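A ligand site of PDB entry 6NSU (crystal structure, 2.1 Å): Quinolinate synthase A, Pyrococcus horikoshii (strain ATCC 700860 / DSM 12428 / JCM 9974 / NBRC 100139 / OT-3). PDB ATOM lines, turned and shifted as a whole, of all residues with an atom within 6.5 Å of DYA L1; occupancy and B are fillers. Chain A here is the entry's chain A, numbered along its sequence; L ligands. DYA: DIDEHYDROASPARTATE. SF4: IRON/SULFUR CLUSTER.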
ATOM      1  N   HIS A  21      16.887  -1.547 -30.695  1.00  0.00           N
ATOM      2  CA  HIS A  21      17.251  -1.713 -29.305  1.00  0.00           C
ATOM      3  C   HIS A  21      18.770  -1.604 -29.139  1.00  0.00           C
ATOM      4  O   HIS A  21      19.539  -1.774 -30.089  1.00  0.00           O
ATOM      5  CB  HIS A  21      16.758  -3.058 -28.770  1.00  0.00           C
ATOM      6  CG  HIS A  21      16.926  -3.227 -27.294  1.00  0.00           C
ATOM      7  ND1 HIS A  21      18.000  -3.894 -26.740  1.00  0.00           N
ATOM      8  CD2 HIS A  21      16.162  -2.806 -26.263  1.00  0.00           C
ATOM      9  CE1 HIS A  21      17.885  -3.879 -25.421  1.00  0.00           C
ATOM     10  NE2 HIS A  21      16.785  -3.231 -25.103  1.00  0.00           N
ATOM     11  N   ASN A  22      19.183  -1.291 -27.909  1.00  0.00           N
ATOM     12  CA  ASN A  22      20.614  -1.130 -27.614  1.00  0.00           C
ATOM     13  C   ASN A  22      21.422  -2.387 -27.918  1.00  0.00           C
ATOM     14  O   ASN A  22      22.640  -2.285 -28.108  1.00  0.00           O
ATOM     15  CB  ASN A  22      20.799  -0.731 -26.152  1.00  0.00           C
ATOM     16  CG  ASN A  22      20.278   0.672 -25.866  1.00  0.00           C
ATOM     17  OD1 ASN A  22      20.398   1.564 -26.699  1.00  0.00           O
ATOM     18  ND2 ASN A  22      19.718   0.857 -24.679  1.00  0.00           N
ATOM     19  N   TYR A  23      20.780  -3.556 -27.952  1.00  0.00           N
ATOM     20  CA  TYR A  23      21.481  -4.809 -28.218  1.00  0.00           C
ATOM     21  C   TYR A  23      21.611  -5.113 -29.701  1.00  0.00           C
ATOM     22  O   TYR A  23      22.138  -6.182 -30.052  1.00  0.00           O
ATOM     23  CB  TYR A  23      20.761  -5.966 -27.523  1.00  0.00           C
ATOM     24  CG  TYR A  23      20.762  -5.898 -26.007  1.00  0.00           C
ATOM     25  CD1 TYR A  23      21.579  -4.998 -25.325  1.00  0.00           C
ATOM     26  CD2 TYR A  23      19.961  -6.750 -25.261  1.00  0.00           C
ATOM     27  CE1 TYR A  23      21.576  -4.941 -23.942  1.00  0.00           C
ATOM     28  CE2 TYR A  23      19.958  -6.703 -23.879  1.00  0.00           C
ATOM     29  CZ  TYR A  23      20.767  -5.797 -23.227  1.00  0.00           C
ATOM     30  OH  TYR A  23      20.758  -5.749 -21.854  1.00  0.00           O
ATOM     31  N   GLY A  36      17.357   2.777 -28.090  1.00  0.00           N
ATOM     32  CA  GLY A  36      17.127   2.755 -26.660  1.00  0.00           C
ATOM     33  C   GLY A  36      16.540   1.418 -26.244  1.00  0.00           C
ATOM     34  O   GLY A  36      16.630   0.436 -26.977  1.00  0.00           O
ATOM     35  N   ASP A  37      15.958   1.390 -25.049  1.00  0.00           N
ATOM     36  CA  ASP A  37      15.289   0.188 -24.591  1.00  0.00           C
ATOM     37  C   ASP A  37      13.876   0.130 -25.166  1.00  0.00           C
ATOM     38  O   ASP A  37      13.426   1.033 -25.873  1.00  0.00           O
ATOM     39  CB  ASP A  37      15.299   0.113 -23.066  1.00  0.00           C
ATOM     40  CG  ASP A  37      14.764   1.369 -22.412  1.00  0.00           C
ATOM     41  OD1 ASP A  37      13.611   1.753 -22.697  1.00  0.00           O
ATOM     42  OD2 ASP A  37      15.498   1.976 -21.593  1.00  0.00           O
ATOM     43  N   SER A  38      13.157  -0.960 -24.854  1.00  0.00           N
ATOM     44  CA  SER A  38      11.905  -1.253 -25.550  1.00  0.00           C
ATOM     45  C   SER A  38      10.844  -0.194 -25.272  1.00  0.00           C
ATOM     46  O   SER A  38      10.246   0.357 -26.198  1.00  0.00           O
ATOM     47  CB  SER A  38      11.396  -2.631 -25.132  1.00  0.00           C
ATOM     48  OG  SER A  38      11.088  -2.676 -23.749  1.00  0.00           O
ATOM     49  N   VAL A  58      13.311  -7.635 -30.602  1.00  0.00           N
ATOM     50  CA  VAL A  58      12.708  -8.954 -30.440  1.00  0.00           C
ATOM     51  C   VAL A  58      11.190  -8.823 -30.461  1.00  0.00           C
ATOM     52  O   VAL A  58      10.654  -7.726 -30.638  1.00  0.00           O
ATOM     53  CB  VAL A  58      13.192  -9.631 -29.148  1.00  0.00           C
ATOM     54  CG1 VAL A  58      14.640 -10.071 -29.296  1.00  0.00           C
ATOM     55  CG2 VAL A  58      13.055  -8.685 -27.970  1.00  0.00           C
ATOM     56  N   PHE A  60       8.482  -9.292 -28.301  1.00  0.00           N
ATOM     57  CA  PHE A  60       7.653  -8.568 -27.339  1.00  0.00           C
ATOM     58  C   PHE A  60       7.838  -7.062 -27.464  1.00  0.00           C
ATOM     59  O   PHE A  60       6.920  -6.293 -27.145  1.00  0.00           O
ATOM     60  CB  PHE A  60       7.966  -9.033 -25.909  1.00  0.00           C
ATOM     61  CG  PHE A  60       9.241  -8.469 -25.336  1.00  0.00           C
ATOM     62  CD1 PHE A  60       9.255  -7.239 -24.699  1.00  0.00           C
ATOM     63  CD2 PHE A  60      10.419  -9.191 -25.425  1.00  0.00           C
ATOM     64  CE1 PHE A  60      10.424  -6.718 -24.181  1.00  0.00           C
ATOM     65  CE2 PHE A  60      11.591  -8.683 -24.887  1.00  0.00           C
ATOM     66  CZ  PHE A  60      11.602  -7.450 -24.271  1.00  0.00           C
ATOM     67  N   MET A  61       9.012  -6.618 -27.918  1.00  0.00           N
ATOM     68  CA  MET A  61       9.246  -5.197 -28.090  1.00  0.00           C
ATOM     69  C   MET A  61       8.393  -4.634 -29.229  1.00  0.00           C
ATOM     70  O   MET A  61       7.761  -3.575 -29.089  1.00  0.00           O
ATOM     71  CB  MET A  61      10.731  -4.943 -28.346  1.00  0.00           C
ATOM     72  CG  MET A  61      11.629  -5.450 -27.240  1.00  0.00           C
ATOM     73  SD  MET A  61      13.374  -5.071 -27.522  1.00  0.00           S
ATOM     74  CE  MET A  61      14.058  -5.511 -25.917  1.00  0.00           C
ATOM     75  N   CYS A  83      12.415 -13.396 -27.574  1.00  0.00           N
ATOM     76  CA  CYS A  83      12.988 -13.332 -26.234  1.00  0.00           C
ATOM     77  C   CYS A  83      12.710 -14.659 -25.539  1.00  0.00           C
ATOM     78  O   CYS A  83      11.552 -15.004 -25.279  1.00  0.00           O
ATOM     79  CB  CYS A  83      12.397 -12.167 -25.444  1.00  0.00           C
ATOM     80  SG  CYS A  83      12.811 -12.175 -23.687  1.00  0.00           S
ATOM     81  N   MET A  85      13.226 -15.470 -22.537  1.00  0.00           N
ATOM     82  CA  MET A  85      12.692 -15.308 -21.188  1.00  0.00           C
ATOM     83  C   MET A  85      11.204 -15.007 -21.192  1.00  0.00           C
ATOM     84  O   MET A  85      10.461 -15.547 -20.366  1.00  0.00           O
ATOM     85  CB  MET A  85      13.456 -14.202 -20.463  1.00  0.00           C
ATOM     86  CG  MET A  85      13.107 -14.088 -18.992  1.00  0.00           C
ATOM     87  SD  MET A  85      13.695 -12.557 -18.266  1.00  0.00           S
ATOM     88  CE  MET A  85      12.322 -11.475 -18.626  1.00  0.00           C
ATOM     89  N   TYR A 109       7.115  -7.766 -15.908  1.00  0.00           N
ATOM     90  CA  TYR A 109       8.188  -7.153 -16.683  1.00  0.00           C
ATOM     91  C   TYR A 109       7.718  -6.891 -18.107  1.00  0.00           C
ATOM     92  O   TYR A 109       6.871  -7.611 -18.644  1.00  0.00           O
ATOM     93  CB  TYR A 109       9.401  -8.091 -16.681  1.00  0.00           C
ATOM     94  CG  TYR A 109      10.746  -7.463 -16.943  1.00  0.00           C
ATOM     95  CD1 TYR A 109      10.883  -6.084 -17.104  1.00  0.00           C
ATOM     96  CD2 TYR A 109      11.893  -8.246 -17.032  1.00  0.00           C
ATOM     97  CE1 TYR A 109      12.129  -5.519 -17.343  1.00  0.00           C
ATOM     98  CE2 TYR A 109      13.131  -7.692 -17.268  1.00  0.00           C
ATOM     99  CZ  TYR A 109      13.238  -6.334 -17.423  1.00  0.00           C
ATOM    100  OH  TYR A 109      14.476  -5.781 -17.658  1.00  0.00           O
ATOM    101  N   ASN A 111       9.387  -7.416 -20.663  1.00  0.00           N
ATOM    102  CA  ASN A 111       9.788  -8.620 -21.400  1.00  0.00           C
ATOM    103  C   ASN A 111       8.746  -9.708 -21.171  1.00  0.00           C
ATOM    104  O   ASN A 111       8.942 -10.659 -20.417  1.00  0.00           O
ATOM    105  CB  ASN A 111      11.176  -9.067 -20.957  1.00  0.00           C
ATOM    106  CG  ASN A 111      12.208  -7.969 -21.055  1.00  0.00           C
ATOM    107  OD1 ASN A 111      11.886  -6.783 -20.939  1.00  0.00           O
ATOM    108  ND2 ASN A 111      13.469  -8.348 -21.273  1.00  0.00           N
ATOM    109  N   SER A 126      13.028  -2.432 -16.137  1.00  0.00           N
ATOM    110  CA  SER A 126      14.132  -2.578 -15.208  1.00  0.00           C
ATOM    111  C   SER A 126      14.624  -1.254 -14.655  1.00  0.00           C
ATOM    112  O   SER A 126      15.580  -1.248 -13.869  1.00  0.00           O
ATOM    113  CB  SER A 126      15.289  -3.324 -15.886  1.00  0.00           C
ATOM    114  OG  SER A 126      15.371  -2.989 -17.253  1.00  0.00           O
ATOM    115  N   ALA A 127      14.011  -0.138 -15.033  1.00  0.00           N
ATOM    116  CA  ALA A 127      14.375   1.173 -14.528  1.00  0.00           C
ATOM    117  C   ALA A 127      13.372   1.752 -13.541  1.00  0.00           C
ATOM    118  O   ALA A 127      13.765   2.534 -12.680  1.00  0.00           O
ATOM    119  CB  ALA A 127      14.538   2.166 -15.695  1.00  0.00           C
ATOM    120  N   CYS A 170      16.940 -14.887 -17.855  1.00  0.00           N
ATOM    121  CA  CYS A 170      17.540 -14.572 -19.142  1.00  0.00           C
ATOM    122  C   CYS A 170      18.878 -15.293 -19.244  1.00  0.00           C
ATOM    123  O   CYS A 170      19.764 -15.092 -18.406  1.00  0.00           O
ATOM    124  CB  CYS A 170      17.732 -13.071 -19.310  1.00  0.00           C
ATOM    125  SG  CYS A 170      18.941 -12.608 -20.569  1.00  0.00           S
ATOM    126  N   HIS A 173      22.199 -12.858 -19.589  1.00  0.00           N
ATOM    127  CA  HIS A 173      22.716 -12.285 -18.344  1.00  0.00           C
ATOM    128  C   HIS A 173      23.027 -13.341 -17.293  1.00  0.00           C
ATOM    129  O   HIS A 173      23.750 -13.056 -16.343  1.00  0.00           O
ATOM    130  CB  HIS A 173      21.718 -11.268 -17.784  1.00  0.00           C
ATOM    131  CG  HIS A 173      21.534 -10.059 -18.642  1.00  0.00           C
ATOM    132  ND1 HIS A 173      20.625 -10.008 -19.672  1.00  0.00           N
ATOM    133  CD2 HIS A 173      22.167  -8.866 -18.635  1.00  0.00           C
ATOM    134  CE1 HIS A 173      20.700  -8.818 -20.258  1.00  0.00           C
ATOM    135  NE2 HIS A 173      21.625  -8.110 -19.643  1.00  0.00           N
ATOM    136  N   HIS A 196      23.602  -5.360 -15.140  1.00  0.00           N
ATOM    137  CA  HIS A 196      22.173  -5.356 -15.388  1.00  0.00           C
ATOM    138  C   HIS A 196      21.443  -6.091 -14.269  1.00  0.00           C
ATOM    139  O   HIS A 196      21.941  -7.096 -13.758  1.00  0.00           O
ATOM    140  CB  HIS A 196      21.866  -6.016 -16.731  1.00  0.00           C
ATOM    141  CG  HIS A 196      20.529  -5.649 -17.307  1.00  0.00           C
ATOM    142  ND1 HIS A 196      19.349  -6.231 -16.883  1.00  0.00           N
ATOM    143  CD2 HIS A 196      20.192  -4.777 -18.281  1.00  0.00           C
ATOM    144  CE1 HIS A 196      18.343  -5.718 -17.557  1.00  0.00           C
ATOM    145  NE2 HIS A 196      18.821  -4.840 -18.419  1.00  0.00           N
ATOM    146  N   GLU A 198      19.185  -8.112 -14.438  1.00  0.00           N
ATOM    147  CA  GLU A 198      18.853  -9.467 -14.850  1.00  0.00           C
ATOM    148  C   GLU A 198      19.950 -10.461 -14.543  1.00  0.00           C
ATOM    149  O   GLU A 198      19.774 -11.656 -14.806  1.00  0.00           O
ATOM    150  CB  GLU A 198      18.511  -9.507 -16.346  1.00  0.00           C
ATOM    151  CG  GLU A 198      17.192  -8.840 -16.707  1.00  0.00           C
ATOM    152  CD  GLU A 198      16.856  -8.985 -18.174  1.00  0.00           C
ATOM    153  OE1 GLU A 198      17.558  -9.728 -18.880  1.00  0.00           O
ATOM    154  OE2 GLU A 198      15.877  -8.353 -18.629  1.00  0.00           O
ATOM    155  N   ALA A 211      21.598  -1.023 -13.126  1.00  0.00           N
ATOM    156  CA  ALA A 211      20.648  -0.261 -13.911  1.00  0.00           C
ATOM    157  C   ALA A 211      20.394  -0.974 -15.237  1.00  0.00           C
ATOM    158  O   ALA A 211      21.177  -1.829 -15.661  1.00  0.00           O
ATOM    159  CB  ALA A 211      21.142   1.163 -14.165  1.00  0.00           C
ATOM    160  N   SER A 212      19.290  -0.600 -15.863  1.00  0.00           N
ATOM    161  CA  SER A 212      18.973  -1.057 -17.206  1.00  0.00           C
ATOM    162  C   SER A 212      19.932  -0.409 -18.215  1.00  0.00           C
ATOM    163  O   SER A 212      20.774   0.410 -17.868  1.00  0.00           O
ATOM    164  CB  SER A 212      17.520  -0.736 -17.550  1.00  0.00           C
ATOM    165  OG  SER A 212      17.280   0.656 -17.460  1.00  0.00           O
ATOM    166  N   THR A 213      19.783  -0.787 -19.479  1.00  0.00           N
ATOM    167  CA  THR A 213      20.611  -0.185 -20.526  1.00  0.00           C
ATOM    168  C   THR A 213      20.352   1.316 -20.627  1.00  0.00           C
ATOM    169  O   THR A 213      21.275   2.094 -20.882  1.00  0.00           O
ATOM    170  CB  THR A 213      20.354  -0.864 -21.870  1.00  0.00           C
ATOM    171  OG1 THR A 213      18.995  -0.646 -22.269  1.00  0.00           O
ATOM    172  CG2 THR A 213      20.610  -2.357 -21.753  1.00  0.00           C
ATOM    173  N   GLY A 214      19.099   1.736 -20.409  1.00  0.00           N
ATOM    174  CA  GLY A 214      18.811   3.155 -20.368  1.00  0.00           C
ATOM    175  C   GLY A 214      19.431   3.824 -19.154  1.00  0.00           C
ATOM    176  O   GLY A 214      19.878   4.979 -19.231  1.00  0.00           O
ATOM    177  N   GLY A 215      19.455   3.130 -18.024  1.00  0.00           N
ATOM    178  CA  GLY A 215      20.091   3.683 -16.839  1.00  0.00           C
ATOM    179  C   GLY A 215      21.601   3.712 -16.949  1.00  0.00           C
ATOM    180  O   GLY A 215      22.256   4.628 -16.433  1.00  0.00           O
ATOM    181  N   THR A 230      26.355  -6.851 -19.410  1.00  0.00           N
ATOM    182  CA  THR A 230      25.110  -7.068 -20.136  1.00  0.00           C
ATOM    183  C   THR A 230      25.473  -7.537 -21.534  1.00  0.00           C
ATOM    184  O   THR A 230      26.622  -7.908 -21.809  1.00  0.00           O
ATOM    185  CB  THR A 230      24.246  -5.795 -20.146  1.00  0.00           C
ATOM    186  OG1 THR A 230      22.959  -6.099 -20.697  1.00  0.00           O
ATOM    187  CG2 THR A 230      24.903  -4.699 -20.978  1.00  0.00           C
ATOM    188  N   CYS A 256      22.674 -12.131 -27.443  1.00  0.00           N
ATOM    189  CA  CYS A 256      21.296 -12.587 -27.524  1.00  0.00           C
ATOM    190  C   CYS A 256      21.010 -13.052 -28.950  1.00  0.00           C
ATOM    191  O   CYS A 256      21.090 -12.264 -29.894  1.00  0.00           O
ATOM    192  CB  CYS A 256      20.329 -11.476 -27.120  1.00  0.00           C
ATOM    193  SG  CYS A 256      18.601 -11.842 -27.472  1.00  0.00           S
ATOM    194  N   MET A 259      18.206 -11.119 -30.632  1.00  0.00           N
ATOM    195  CA  MET A 259      18.619  -9.820 -31.131  1.00  0.00           C
ATOM    196  C   MET A 259      19.417  -9.949 -32.425  1.00  0.00           C
ATOM    197  O   MET A 259      19.256  -9.145 -33.346  1.00  0.00           O
ATOM    198  CB  MET A 259      19.436  -9.075 -30.079  1.00  0.00           C
ATOM    199  CG  MET A 259      18.607  -8.508 -28.944  1.00  0.00           C
ATOM    200  SD  MET A 259      17.452  -7.251 -29.527  1.00  0.00           S
ATOM    201  CE  MET A 259      16.676  -6.784 -27.990  1.00  0.00           C
HETATM  202  N   DYA L   1      16.358  -5.182 -20.159  1.00  0.00           N
HETATM  203  CA  DYA L   1      16.724  -4.569 -21.350  1.00  0.00           C
HETATM  204  CB  DYA L   1      16.820  -5.200 -22.539  1.00  0.00           C
HETATM  205  CG  DYA L   1      16.504  -6.680 -22.588  1.00  0.00           C
HETATM  206  OD1 DYA L   1      16.587  -7.248 -23.661  1.00  0.00           O
HETATM  207  OD2 DYA L   1      16.168  -7.332 -21.607  1.00  0.00           O
HETATM  208  C   DYA L   1      17.043  -3.097 -21.317  1.00  0.00           C
HETATM  209  O   DYA L   1      16.960  -2.421 -20.155  1.00  0.00           O
HETATM  210  OXT DYA L   1      17.376  -2.520 -22.332  1.00  0.00           O
HETATM  211 FE1  SF4 L   2      16.881  -9.194 -23.416  1.00  0.00          FE
HETATM  212 FE2  SF4 L   2      15.026 -11.617 -23.875  1.00  0.00          FE
HETATM  213 FE3  SF4 L   2      17.705 -11.985 -22.390  1.00  0.00          FE
HETATM  214 FE4  SF4 L   2      17.692 -11.402 -25.418  1.00  0.00          FE
HETATM  215  S1  SF4 L   2      16.773 -12.921 -24.125  1.00  0.00           S
HETATM  216  S2  SF4 L   2      18.630 -10.477 -23.677  1.00  0.00           S
HETATM  217  S3  SF4 L   2      15.945 -10.108 -25.170  1.00  0.00           S
HETATM  218  S4  SF4 L   2      15.953 -10.705 -22.115  1.00  0.00           S
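A nitrogen (N) of DYA L1 sits at hydrogen-bond distance from a ring nitrogen (NE2) of His 196, 3.0 Å away.
The side-chain sulfur of Cys 256 is bound to an iron atom (FE4) of SF4 L2, 2.3 Å away.
ND2 of Asn 111 lies within hydrogen-bond range of OD2 of DYA L1, at 2.9 Å.
The side-chain amide nitrogen (ND2) of Asn 111 lies close to a sulfur (S4) of SF4 L2 (3.5 Å).
The side-chain sulfur of Cys 170 binds an iron atom (FE3) of SF4 L2.
The side-chain hydroxyl of Tyr 109 sits at hydrogen-bond distance from a nitrogen (N) of DYA L1, 3.2 Å away.
A ring nitrogen (NE2) of His 21 lies within hydrogen-bond range of an oxygen (OXT) of DYA L1.
The backbone NH (N) of Thr 213 is in hydrogen-bond range of an oxygen (O) of DYA L1, 3.3 Å away.
An oxygen (OXT) of DYA L1 sits at hydrogen-bond distance from the side-chain hydroxyl of Thr 213, at 2.5 Å.
The side-chain sulfur of Cys 83 is bound to an iron atom (FE2) of SF4 L2, 2.3 Å away.
An oxygen (O) of DYA L1 is in hydrogen-bond range of the side-chain hydroxyl (OG) of Ser 126 (3.4 Å).
An iron atom (FE1) of SF4 L2 is bound by an oxygen (OD1) of DYA L1, at 2.0 Å.
The side-chain carboxylate (OE1) of Glu 198 lies close to the side-chain sulfur (SG) of Cys 170, 3.6 Å away.
A ring nitrogen (ND1) of His 196 sits close to the backbone NH (N) of Glu 198, 3.1 Å away.
The side-chain hydroxyl of Tyr 109 is in hydrogen-bond range of the side-chain hydroxyl of Ser 126, at 3.0 Å.
The side-chain carboxylate (OE1) of Glu 198 is in hydrogen-bond range of a ring nitrogen (ND1) of His 173.
OE2 of Glu 198 is in hydrogen-bond range of OH of Tyr 109, 3.1 Å away.
The side-chain hydroxyl of Tyr 23 sits at hydrogen-bond distance from a ring nitrogen (NE2) of His 173 (3.3 Å).
N of Gly 215 sits at hydrogen-bond distance from OG of Ser 212, at 3.3 Å.
OH of Tyr 23 lies within hydrogen-bond range of OG1 of Thr 230 (2.5 Å).
An oxygen (OD2) of DYA L1 lies close to the side-chain carboxylate (OE2) of Glu 198 (3.2 Å).
Tyr 23 touches DYA L1 (CE2 to OD1, 3.4 Å).
Asp 37 touches DYA L1.
Met 61 touches DYA L1 (CE to OD1, 3.8 Å).
Ser 212 touches DYA L1 (CB to O, 3.2 Å).
Hydrophobic or aromatic side chains that line DYA L1: His 21, Tyr 23, Met 61 and His 196.
11 residues have an atom within 4 Å of DYA L1: His 21, Tyr 23, Asp 37, Met 61, Tyr 109, Asn 111, Ser 126, His 196, Glu 198, Ser 212 and Thr 213.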
